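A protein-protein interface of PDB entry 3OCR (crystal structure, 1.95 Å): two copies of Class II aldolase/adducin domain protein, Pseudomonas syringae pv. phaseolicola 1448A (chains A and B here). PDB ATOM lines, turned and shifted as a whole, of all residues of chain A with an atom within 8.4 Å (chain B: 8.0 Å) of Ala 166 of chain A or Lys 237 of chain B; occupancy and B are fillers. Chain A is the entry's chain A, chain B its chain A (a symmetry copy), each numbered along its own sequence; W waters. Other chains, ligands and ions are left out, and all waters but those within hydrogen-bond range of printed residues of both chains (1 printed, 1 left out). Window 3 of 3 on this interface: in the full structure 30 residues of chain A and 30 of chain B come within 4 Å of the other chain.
No position is printed for both chains.
Ala 166 of chain A touches just these residues of chain B: Lys 237 and Gln 241. Of the printed residues of chain A, Lys 237 of chain B touches Glu 163 (2.8 Å), Gly 164 (3.7 Å) and Ala 166 (3.4 Å). No residue of chain A comes within 4 Å of Ala 236 of chain B. Of the printed residues of chain B, Tyr 162 of chain A touches Gln 148 (2.6 Å), Ile 151 (3.98 Å), Val 234 (3.7 Å) and Val 238 (3.8 Å). Printed residues of chain B within 4 Å of Glu 163 of chain A: Val 234 and Lys 237. Printed residues of chain A within 4 Å of Ile 151 of chain B: Tyr 162. Of the printed residues of chain A, Val 238 of chain B touches Tyr 162, Gly 164 and Ile 165. The nearest residue of chain B that does not touch Ala 166 of chain A is Gln 148 of chain B (6.0 Å). The nearest residue of chain A that does not touch Lys 237 of chain B is Ile 165 of chain A (4.2 Å).
Water W1 bridges the backbone carbonyl oxygen of His 190 of chain A and the backbone NH of Gln 148 of chain B.
Printed residues of chain A that touch a printed residue of chain B: Tyr 162, Glu 163, Gly 164, Ile 165, Ala 166 and His 190. Hydrophobic or aromatic side chains of chain A within 4 Å of the printed part of chain B: Tyr 162, Ile 165, Ala 166 and His 190. Of the 15 printed residues of chain B, 6 touch a printed residue of chain A. Among the printed residues, 17 pairs touch across the chains. Among the printed residues, no Asp or Glu carboxylate lies within 4 Å of a Lys or Arg side-chain nitrogen of the other chain.
N of Ile 165 of chain A sits close to NE2 of Gln 241 of chain B, 2.9 Å away. The side-chain hydroxyl (OH) of Tyr 162 of chain A sits at hydrogen-bond distance from the side-chain amide nitrogen (NE2) of Gln 148 of chain B (2.6 Å). The side-chain amino group (NZ) of Lys 237 of chain B is in hydrogen-bond range of the backbone carbonyl oxygen (O) of Glu 163 of chain A (2.8 Å). The backbone NH (N) of Ala 166 of chain A lies within hydrogen-bond range of the side-chain amide oxygen (OE1) of Gln 241 of chain B, 3.5 Å away. The side-chain amino group (NZ) of Lys 237 of chain B is in hydrogen-bond range of the backbone carbonyl oxygen (O) of Ala 166 of chain A, 3.4 Å away.
The side-chain amide oxygen of Gln 241 of chain B lies within hydrogen-bond range of the side-chain amino group of Lys 237 of chain B, 3.0 Å away.
Among the printed residues, merely in contact across the chains: Tyr 162 of chain A with Ile 151 of chain B, Tyr 162 of chain A with Val 234 of chain B, Tyr 162 of chain A with Val 238 of chain B, Glu 163 of chain A with Val 234 of chain B, Gly 164 of chain A with Gln 148 of chain B, Gly 164 of chain A with Val 234 of chain B, Gly 164 of chain A with Lys 237 of chain B, Gly 164 of chain A with Val 238 of chain B, Gly 164 of chain A with Gln 241 of chain B, Ile 165 of chain A with Gln 148 of chain B, Ile 165 of chain A with Val 238 of chain B and His 190 of chain A with Gln 148 of chain B.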
ATOM      1  N   ALA A 107     -17.208 -26.556  -9.428  1.00  0.00           N
ATOM      2  CA  ALA A 107     -16.376 -25.765  -8.521  1.00  0.00           C
ATOM      3  C   ALA A 107     -17.057 -24.450  -8.110  1.00  0.00           C
ATOM      4  O   ALA A 107     -16.883 -23.977  -6.981  1.00  0.00           O
ATOM      5  CB  ALA A 107     -15.019 -25.501  -9.157  1.00  0.00           C
ATOM      6  N   GLY A 108     -17.836 -23.868  -9.024  1.00  0.00           N
ATOM      7  CA  GLY A 108     -18.585 -22.637  -8.732  1.00  0.00           C
ATOM      8  C   GLY A 108     -19.736 -22.835  -7.748  1.00  0.00           C
ATOM      9  O   GLY A 108     -20.205 -21.881  -7.141  1.00  0.00           O
ATOM     10  N   VAL A 110     -19.662 -24.783  -4.978  1.00  0.00           N
ATOM     11  CA  VAL A 110     -19.197 -25.008  -3.614  1.00  0.00           C
ATOM     12  C   VAL A 110     -19.607 -23.907  -2.627  1.00  0.00           C
ATOM     13  O   VAL A 110     -20.037 -24.201  -1.511  1.00  0.00           O
ATOM     14  CB  VAL A 110     -17.675 -25.225  -3.585  1.00  0.00           C
ATOM     15  CG1 VAL A 110     -17.152 -25.216  -2.139  1.00  0.00           C
ATOM     16  CG2 VAL A 110     -17.320 -26.564  -4.297  1.00  0.00           C
ATOM     17  N   ILE A 111     -19.484 -22.646  -3.027  1.00  0.00           N
ATOM     18  CA  ILE A 111     -19.901 -21.557  -2.136  1.00  0.00           C
ATOM     19  C   ILE A 111     -21.400 -21.617  -1.812  1.00  0.00           C
ATOM     20  O   ILE A 111     -21.796 -21.449  -0.673  1.00  0.00           O
ATOM     21  CB  ILE A 111     -19.462 -20.151  -2.651  1.00  0.00           C
ATOM     22  CG1 ILE A 111     -19.776 -19.091  -1.590  1.00  0.00           C
ATOM     23  CG2 ILE A 111     -20.075 -19.819  -4.039  1.00  0.00           C
ATOM     24  CD1 ILE A 111     -18.838 -17.891  -1.626  1.00  0.00           C
ATOM     25  N   HIS A 160     -15.519 -11.261   4.398  1.00  0.00           N
ATOM     26  CA  HIS A 160     -14.740 -12.490   4.298  1.00  0.00           C
ATOM     27  C   HIS A 160     -13.455 -12.175   3.504  1.00  0.00           C
ATOM     28  O   HIS A 160     -13.518 -11.770   2.334  1.00  0.00           O
ATOM     29  CB  HIS A 160     -15.592 -13.595   3.620  1.00  0.00           C
ATOM     30  CG  HIS A 160     -14.841 -14.865   3.347  1.00  0.00           C
ATOM     31  ND1 HIS A 160     -14.508 -15.765   4.341  1.00  0.00           N
ATOM     32  CD2 HIS A 160     -14.371 -15.389   2.188  1.00  0.00           C
ATOM     33  CE1 HIS A 160     -13.841 -16.774   3.809  1.00  0.00           C
ATOM     34  NE2 HIS A 160     -13.756 -16.577   2.503  1.00  0.00           N
ATOM     35  N   TYR A 162     -10.050 -12.640   1.372  1.00  0.00           N
ATOM     36  CA  TYR A 162      -9.813 -13.417   0.159  1.00  0.00           C
ATOM     37  C   TYR A 162      -8.795 -14.539   0.368  1.00  0.00           C
ATOM     38  O   TYR A 162      -7.697 -14.310   0.907  1.00  0.00           O
ATOM     39  CB  TYR A 162      -9.344 -12.521  -0.993  1.00  0.00           C
ATOM     40  CG  TYR A 162      -9.366 -13.236  -2.343  1.00  0.00           C
ATOM     41  CD1 TYR A 162     -10.545 -13.796  -2.840  1.00  0.00           C
ATOM     42  CD2 TYR A 162      -8.187 -13.388  -3.099  1.00  0.00           C
ATOM     43  CE1 TYR A 162     -10.568 -14.475  -4.086  1.00  0.00           C
ATOM     44  CE2 TYR A 162      -8.197 -14.064  -4.324  1.00  0.00           C
ATOM     45  CZ  TYR A 162      -9.398 -14.587  -4.813  1.00  0.00           C
ATOM     46  OH  TYR A 162      -9.371 -15.269  -6.012  1.00  0.00           O
ATOM     47  N   GLU A 163      -9.139 -15.738  -0.089  1.00  0.00           N
ATOM     48  CA  GLU A 163      -8.219 -16.875   0.064  1.00  0.00           C
ATOM     49  C   GLU A 163      -7.888 -17.622  -1.242  1.00  0.00           C
ATOM     50  O   GLU A 163      -7.151 -18.589  -1.227  1.00  0.00           O
ATOM     51  CB  GLU A 163      -8.722 -17.843   1.143  1.00  0.00           C
ATOM     52  CG  GLU A 163      -9.007 -17.171   2.491  1.00  0.00           C
ATOM     53  CD  GLU A 163      -9.281 -18.172   3.597  1.00  0.00           C
ATOM     54  OE1 GLU A 163      -8.609 -19.229   3.628  1.00  0.00           O
ATOM     55  OE2 GLU A 163     -10.169 -17.904   4.438  1.00  0.00           O
ATOM     56  N   GLY A 164      -8.419 -17.157  -2.365  1.00  0.00           N
ATOM     57  CA  GLY A 164      -8.074 -17.744  -3.657  1.00  0.00           C
ATOM     58  C   GLY A 164      -9.340 -18.176  -4.353  1.00  0.00           C
ATOM     59  O   GLY A 164     -10.437 -17.870  -3.891  1.00  0.00           O
ATOM     60  N   ILE A 165      -9.183 -18.899  -5.456  1.00  0.00           N
ATOM     61  CA  ILE A 165     -10.333 -19.255  -6.304  1.00  0.00           C
ATOM     62  C   ILE A 165     -11.127 -20.420  -5.701  1.00  0.00           C
ATOM     63  O   ILE A 165     -12.328 -20.299  -5.483  1.00  0.00           O
ATOM     64  CB  ILE A 165      -9.899 -19.548  -7.769  1.00  0.00           C
ATOM     65  CG1 ILE A 165      -9.259 -18.295  -8.393  1.00  0.00           C
ATOM     66  CG2 ILE A 165     -11.099 -20.032  -8.611  1.00  0.00           C
ATOM     67  CD1 ILE A 165      -8.523 -18.536  -9.726  1.00  0.00           C
ATOM     68  N   ALA A 166     -10.446 -21.528  -5.423  1.00  0.00           N
ATOM     69  CA  ALA A 166     -11.090 -22.728  -4.900  1.00  0.00           C
ATOM     70  C   ALA A 166     -11.354 -22.568  -3.416  1.00  0.00           C
ATOM     71  O   ALA A 166     -10.535 -22.021  -2.673  1.00  0.00           O
ATOM     72  CB  ALA A 166     -10.232 -23.978  -5.157  1.00  0.00           C
ATOM     73  N   LEU A 167     -12.518 -23.047  -2.998  1.00  0.00           N
ATOM     74  CA  LEU A 167     -12.939 -22.946  -1.621  1.00  0.00           C
ATOM     75  C   LEU A 167     -12.689 -24.297  -0.925  1.00  0.00           C
ATOM     76  O   LEU A 167     -13.498 -25.219  -1.033  1.00  0.00           O
ATOM     77  CB  LEU A 167     -14.413 -22.536  -1.593  1.00  0.00           C
ATOM     78  CG  LEU A 167     -15.182 -22.293  -0.292  1.00  0.00           C
ATOM     79  CD1 LEU A 167     -14.497 -21.293   0.614  1.00  0.00           C
ATOM     80  CD2 LEU A 167     -16.575 -21.805  -0.641  1.00  0.00           C
ATOM     81  N   ASP A 168     -11.541 -24.415  -0.257  1.00  0.00           N
ATOM     82  CA  ASP A 168     -11.224 -25.629   0.494  1.00  0.00           C
ATOM     83  C   ASP A 168     -11.946 -25.609   1.834  1.00  0.00           C
ATOM     84  O   ASP A 168     -12.546 -24.599   2.212  1.00  0.00           O
ATOM     85  CB  ASP A 168      -9.699 -25.884   0.639  1.00  0.00           C
ATOM     86  CG  ASP A 168      -8.988 -24.937   1.637  1.00  0.00           C
ATOM     87  OD1 ASP A 168      -9.541 -24.595   2.715  1.00  0.00           O
ATOM     88  OD2 ASP A 168      -7.828 -24.561   1.344  1.00  0.00           O
ATOM     89  N   LEU A 169     -11.882 -26.738   2.524  1.00  0.00           N
ATOM     90  CA  LEU A 169     -12.596 -26.974   3.768  1.00  0.00           C
ATOM     91  C   LEU A 169     -12.269 -25.949   4.844  1.00  0.00           C
ATOM     92  O   LEU A 169     -13.164 -25.469   5.530  1.00  0.00           O
ATOM     93  CB  LEU A 169     -12.249 -28.374   4.273  1.00  0.00           C
ATOM     94  CG  LEU A 169     -13.153 -29.012   5.321  1.00  0.00           C
ATOM     95  CD1 LEU A 169     -14.567 -29.255   4.776  1.00  0.00           C
ATOM     96  CD2 LEU A 169     -12.494 -30.302   5.748  1.00  0.00           C
ATOM     97  N   GLU A 171     -11.256 -22.849   4.385  1.00  0.00           N
ATOM     98  CA  GLU A 171     -11.959 -21.627   4.011  1.00  0.00           C
ATOM     99  C   GLU A 171     -13.485 -21.736   4.106  1.00  0.00           C
ATOM    100  O   GLU A 171     -14.125 -20.767   4.496  1.00  0.00           O
ATOM    101  CB  GLU A 171     -11.568 -21.122   2.615  1.00  0.00           C
ATOM    102  CG  GLU A 171     -12.055 -19.667   2.381  1.00  0.00           C
ATOM    103  CD  GLU A 171     -11.946 -19.186   0.946  1.00  0.00           C
ATOM    104  OE1 GLU A 171     -11.358 -19.912   0.093  1.00  0.00           O
ATOM    105  OE2 GLU A 171     -12.466 -18.070   0.676  1.00  0.00           O
ATOM    106  N   ARG A 172     -14.061 -22.882   3.727  1.00  0.00           N
ATOM    107  CA  ARG A 172     -15.511 -23.094   3.858  1.00  0.00           C
ATOM    108  C   ARG A 172     -15.978 -22.813   5.298  1.00  0.00           C
ATOM    109  O   ARG A 172     -17.007 -22.184   5.506  1.00  0.00           O
ATOM    110  CB  ARG A 172     -15.901 -24.533   3.532  1.00  0.00           C
ATOM    111  CG  ARG A 172     -16.285 -24.886   2.098  1.00  0.00           C
ATOM    112  CD  ARG A 172     -16.623 -26.406   2.096  1.00  0.00           C
ATOM    113  NE  ARG A 172     -16.524 -27.073   0.797  1.00  0.00           N
ATOM    114  CZ  ARG A 172     -15.435 -27.700   0.343  1.00  0.00           C
ATOM    115  NH1 ARG A 172     -14.323 -27.734   1.065  1.00  0.00           N
ATOM    116  NH2 ARG A 172     -15.453 -28.282  -0.852  1.00  0.00           N
ATOM    117  N   HIS A 190     -13.176  -9.781  -4.220  1.00  0.00           N
ATOM    118  CA  HIS A 190     -13.748 -10.906  -4.937  1.00  0.00           C
ATOM    119  C   HIS A 190     -15.097 -10.542  -5.507  1.00  0.00           C
ATOM    120  O   HIS A 190     -15.305 -10.728  -6.708  1.00  0.00           O
ATOM    121  CB  HIS A 190     -13.754 -12.165  -4.025  1.00  0.00           C
ATOM    122  CG  HIS A 190     -14.327 -13.398  -4.665  1.00  0.00           C
ATOM    123  ND1 HIS A 190     -14.471 -14.588  -3.985  1.00  0.00           N
ATOM    124  CD2 HIS A 190     -14.808 -13.620  -5.914  1.00  0.00           C
ATOM    125  CE1 HIS A 190     -14.997 -15.495  -4.794  1.00  0.00           C
ATOM    126  NE2 HIS A 190     -15.223 -14.927  -5.967  1.00  0.00           N
ATOM    127  N   GLN B 148      -9.916 -10.989  -7.807  1.00  0.00           N
ATOM    128  CA  GLN B 148      -9.703 -12.324  -8.375  1.00  0.00           C
ATOM    129  C   GLN B 148      -9.269 -12.243  -9.846  1.00  0.00           C
ATOM    130  O   GLN B 148      -8.403 -12.991 -10.307  1.00  0.00           O
ATOM    131  CB  GLN B 148     -10.966 -13.154  -8.265  1.00  0.00           C
ATOM    132  CG  GLN B 148     -10.815 -14.552  -8.834  1.00  0.00           C
ATOM    133  CD  GLN B 148     -11.836 -15.502  -8.262  1.00  0.00           C
ATOM    134  OE1 GLN B 148     -12.783 -15.916  -8.961  1.00  0.00           O
ATOM    135  NE2 GLN B 148     -11.672 -15.846  -6.985  1.00  0.00           N
ATOM    136  N   ILE B 151      -5.601 -10.876 -10.079  1.00  0.00           N
ATOM    137  CA  ILE B 151      -4.651 -11.768  -9.385  1.00  0.00           C
ATOM    138  C   ILE B 151      -4.387 -13.000 -10.253  1.00  0.00           C
ATOM    139  O   ILE B 151      -3.275 -13.535 -10.272  1.00  0.00           O
ATOM    140  CB  ILE B 151      -5.156 -12.131  -7.939  1.00  0.00           C
ATOM    141  CG1 ILE B 151      -5.166 -10.895  -7.054  1.00  0.00           C
ATOM    142  CG2 ILE B 151      -4.326 -13.242  -7.263  1.00  0.00           C
ATOM    143  CD1 ILE B 151      -6.027 -11.041  -5.743  1.00  0.00           C
ATOM    144  N   PRO B 231      -2.674 -11.422   0.903  1.00  0.00           N
ATOM    145  CA  PRO B 231      -1.293 -11.774   1.215  1.00  0.00           C
ATOM    146  C   PRO B 231      -0.647 -12.476   0.035  1.00  0.00           C
ATOM    147  O   PRO B 231      -1.349 -12.985  -0.859  1.00  0.00           O
ATOM    148  CB  PRO B 231      -1.419 -12.725   2.418  1.00  0.00           C
ATOM    149  CG  PRO B 231      -2.826 -12.652   2.857  1.00  0.00           C
ATOM    150  CD  PRO B 231      -3.629 -12.235   1.674  1.00  0.00           C
ATOM    151  N   ARG B 232       0.678 -12.448   0.020  1.00  0.00           N
ATOM    152  CA  ARG B 232       1.479 -13.022  -1.066  1.00  0.00           C
ATOM    153  C   ARG B 232       1.143 -14.498  -1.327  1.00  0.00           C
ATOM    154  O   ARG B 232       1.038 -14.911  -2.491  1.00  0.00           O
ATOM    155  CB  ARG B 232       2.978 -12.834  -0.771  1.00  0.00           C
ATOM    156  CG  ARG B 232       3.434 -11.371  -0.849  1.00  0.00           C
ATOM    157  CD  ARG B 232       4.057 -11.035  -2.219  1.00  0.00           C
ATOM    158  NE  ARG B 232       3.921  -9.627  -2.619  1.00  0.00           N
ATOM    159  CZ  ARG B 232       4.649  -8.609  -2.149  1.00  0.00           C
ATOM    160  NH1 ARG B 232       5.590  -8.793  -1.225  1.00  0.00           N
ATOM    161  NH2 ARG B 232       4.418  -7.383  -2.604  1.00  0.00           N
ATOM    162  N   GLU B 233       0.971 -15.271  -0.253  1.00  0.00           N
ATOM    163  CA  GLU B 233       0.630 -16.695  -0.357  1.00  0.00           C
ATOM    164  C   GLU B 233      -0.672 -16.905  -1.127  1.00  0.00           C
ATOM    165  O   GLU B 233      -0.785 -17.839  -1.927  1.00  0.00           O
ATOM    166  CB  GLU B 233       0.526 -17.326   1.027  1.00  0.00           C
ATOM    167  CG  GLU B 233       1.617 -16.865   1.991  1.00  0.00           C
ATOM    168  CD  GLU B 233       1.248 -15.574   2.680  1.00  0.00           C
ATOM    169  OE1 GLU B 233       0.492 -15.642   3.673  1.00  0.00           O
ATOM    170  OE2 GLU B 233       1.705 -14.500   2.229  1.00  0.00           O
ATOM    171  N   VAL B 234      -1.644 -16.024  -0.887  1.00  0.00           N
ATOM    172  CA  VAL B 234      -2.952 -16.112  -1.562  1.00  0.00           C
ATOM    173  C   VAL B 234      -2.810 -15.834  -3.060  1.00  0.00           C
ATOM    174  O   VAL B 234      -3.414 -16.524  -3.887  1.00  0.00           O
ATOM    175  CB  VAL B 234      -3.995 -15.181  -0.906  1.00  0.00           C
ATOM    176  CG1 VAL B 234      -5.301 -15.168  -1.711  1.00  0.00           C
ATOM    177  CG2 VAL B 234      -4.235 -15.597   0.543  1.00  0.00           C
ATOM    178  N   ILE B 235      -2.012 -14.819  -3.396  1.00  0.00           N
ATOM    179  CA  ILE B 235      -1.679 -14.500  -4.795  1.00  0.00           C
ATOM    180  C   ILE B 235      -1.031 -15.738  -5.427  1.00  0.00           C
ATOM    181  O   ILE B 235      -1.468 -16.200  -6.497  1.00  0.00           O
ATOM    182  CB  ILE B 235      -0.719 -13.263  -4.900  1.00  0.00           C
ATOM    183  CG1 ILE B 235      -1.316 -12.012  -4.230  1.00  0.00           C
ATOM    184  CG2 ILE B 235      -0.252 -12.997  -6.349  1.00  0.00           C
ATOM    185  CD1 ILE B 235      -2.644 -11.689  -4.675  1.00  0.00           C
ATOM    186  N   ALA B 236      -0.032 -16.279  -4.733  1.00  0.00           N
ATOM    187  CA  ALA B 236       0.683 -17.504  -5.171  1.00  0.00           C
ATOM    188  C   ALA B 236      -0.233 -18.692  -5.449  1.00  0.00           C
ATOM    189  O   ALA B 236      -0.081 -19.354  -6.475  1.00  0.00           O
ATOM    190  CB  ALA B 236       1.731 -17.898  -4.175  1.00  0.00           C
ATOM    191  N   LYS B 237      -1.174 -18.934  -4.540  1.00  0.00           N
ATOM    192  CA  LYS B 237      -2.215 -19.947  -4.729  1.00  0.00           C
ATOM    193  C   LYS B 237      -3.019 -19.721  -6.018  1.00  0.00           C
ATOM    194  O   LYS B 237      -3.248 -20.656  -6.778  1.00  0.00           O
ATOM    195  CB  LYS B 237      -3.134 -20.026  -3.491  1.00  0.00           C
ATOM    196  CG  LYS B 237      -4.266 -21.098  -3.564  1.00  0.00           C
ATOM    197  CD  LYS B 237      -4.693 -21.657  -2.170  1.00  0.00           C
ATOM    198  CE  LYS B 237      -6.179 -22.169  -2.118  1.00  0.00           C
ATOM    199  NZ  LYS B 237      -7.284 -21.097  -2.382  1.00  0.00           N
ATOM    200  N   VAL B 238      -3.454 -18.488  -6.259  1.00  0.00           N
ATOM    201  CA  VAL B 238      -4.232 -18.197  -7.457  1.00  0.00           C
ATOM    202  C   VAL B 238      -3.395 -18.429  -8.719  1.00  0.00           C
ATOM    203  O   VAL B 238      -3.919 -18.905  -9.755  1.00  0.00           O
ATOM    204  CB  VAL B 238      -4.857 -16.792  -7.409  1.00  0.00           C
ATOM    205  CG1 VAL B 238      -5.541 -16.438  -8.758  1.00  0.00           C
ATOM    206  CG2 VAL B 238      -5.880 -16.716  -6.266  1.00  0.00           C
ATOM    207  N   GLU B 239      -2.099 -18.115  -8.619  1.00  0.00           N
ATOM    208  CA  GLU B 239      -1.142 -18.347  -9.701  1.00  0.00           C
ATOM    209  C   GLU B 239      -1.102 -19.831 -10.045  1.00  0.00           C
ATOM    210  O   GLU B 239      -1.089 -20.192 -11.211  1.00  0.00           O
ATOM    211  CB  GLU B 239       0.276 -17.885  -9.325  1.00  0.00           C
ATOM    212  CG  GLU B 239       0.451 -16.385  -9.187  1.00  0.00           C
ATOM    213  CD  GLU B 239       1.914 -15.961  -9.051  1.00  0.00           C
ATOM    214  OE1 GLU B 239       2.823 -16.757  -9.373  1.00  0.00           O
ATOM    215  OE2 GLU B 239       2.150 -14.811  -8.631  1.00  0.00           O
ATOM    216  N   GLU B 240      -1.087 -20.681  -9.017  1.00  0.00           N
ATOM    217  CA  GLU B 240      -1.072 -22.128  -9.220  1.00  0.00           C
ATOM    218  C   GLU B 240      -2.414 -22.603  -9.795  1.00  0.00           C
ATOM    219  O   GLU B 240      -2.442 -23.382 -10.742  1.00  0.00           O
ATOM    220  CB  GLU B 240      -0.710 -22.850  -7.920  1.00  0.00           C
ATOM    221  CG  GLU B 240      -0.336 -24.319  -8.093  1.00  0.00           C
ATOM    222  CD  GLU B 240       0.876 -24.552  -8.987  1.00  0.00           C
ATOM    223  OE1 GLU B 240       1.689 -23.608  -9.174  1.00  0.00           O
ATOM    224  OE2 GLU B 240       1.017 -25.691  -9.493  1.00  0.00           O
ATOM    225  N   GLN B 241      -3.508 -22.090  -9.242  1.00  0.00           N
ATOM    226  CA  GLN B 241      -4.869 -22.359  -9.730  1.00  0.00           C
ATOM    227  C   GLN B 241      -5.080 -21.970 -11.201  1.00  0.00           C
ATOM    228  O   GLN B 241      -5.789 -22.663 -11.935  1.00  0.00           O
ATOM    229  CB  GLN B 241      -5.897 -21.647  -8.832  1.00  0.00           C
ATOM    230  CG  GLN B 241      -6.145 -22.356  -7.480  1.00  0.00           C
ATOM    231  CD  GLN B 241      -6.704 -21.450  -6.371  1.00  0.00           C
ATOM    232  OE1 GLN B 241      -7.020 -21.931  -5.279  1.00  0.00           O
ATOM    233  NE2 GLN B 241      -6.811 -20.146  -6.640  1.00  0.00           N
ATOM    234  N   ALA B 242      -4.467 -20.861 -11.623  1.00  0.00           N
ATOM    235  CA  ALA B 242      -4.557 -20.411 -13.020  1.00  0.00           C
ATOM    236  C   ALA B 242      -3.511 -21.060 -13.937  1.00  0.00           C
ATOM    237  O   ALA B 242      -3.707 -21.090 -15.145  1.00  0.00           O
ATOM    238  CB  ALA B 242      -4.496 -18.879 -13.115  1.00  0.00           C
ATOM    239  N   LYS B 243      -2.412 -21.560 -13.357  1.00  0.00           N
ATOM    240  CA  LYS B 243      -1.324 -22.261 -14.089  1.00  0.00           C
ATOM    241  C   LYS B 243      -1.789 -23.585 -14.700  1.00  0.00           C
ATOM    242  O   LYS B 243      -1.283 -24.015 -15.734  1.00  0.00           O
ATOM    243  CB  LYS B 243      -0.093 -22.463 -13.188  1.00  0.00           C
ATOM    244  CG  LYS B 243       0.811 -23.656 -13.522  1.00  0.00           C
ATOM    245  CD  LYS B 243       2.126 -23.572 -12.748  1.00  0.00           C
ATOM    246  CE  LYS B 243       2.504 -24.908 -12.098  1.00  0.00           C
ATOM    247  NZ  LYS B 243       2.863 -25.992 -13.064  1.00  0.00           N
HETATM  248  O   HOH W   1     -12.909 -10.715  -8.254  1.00  0.00           O
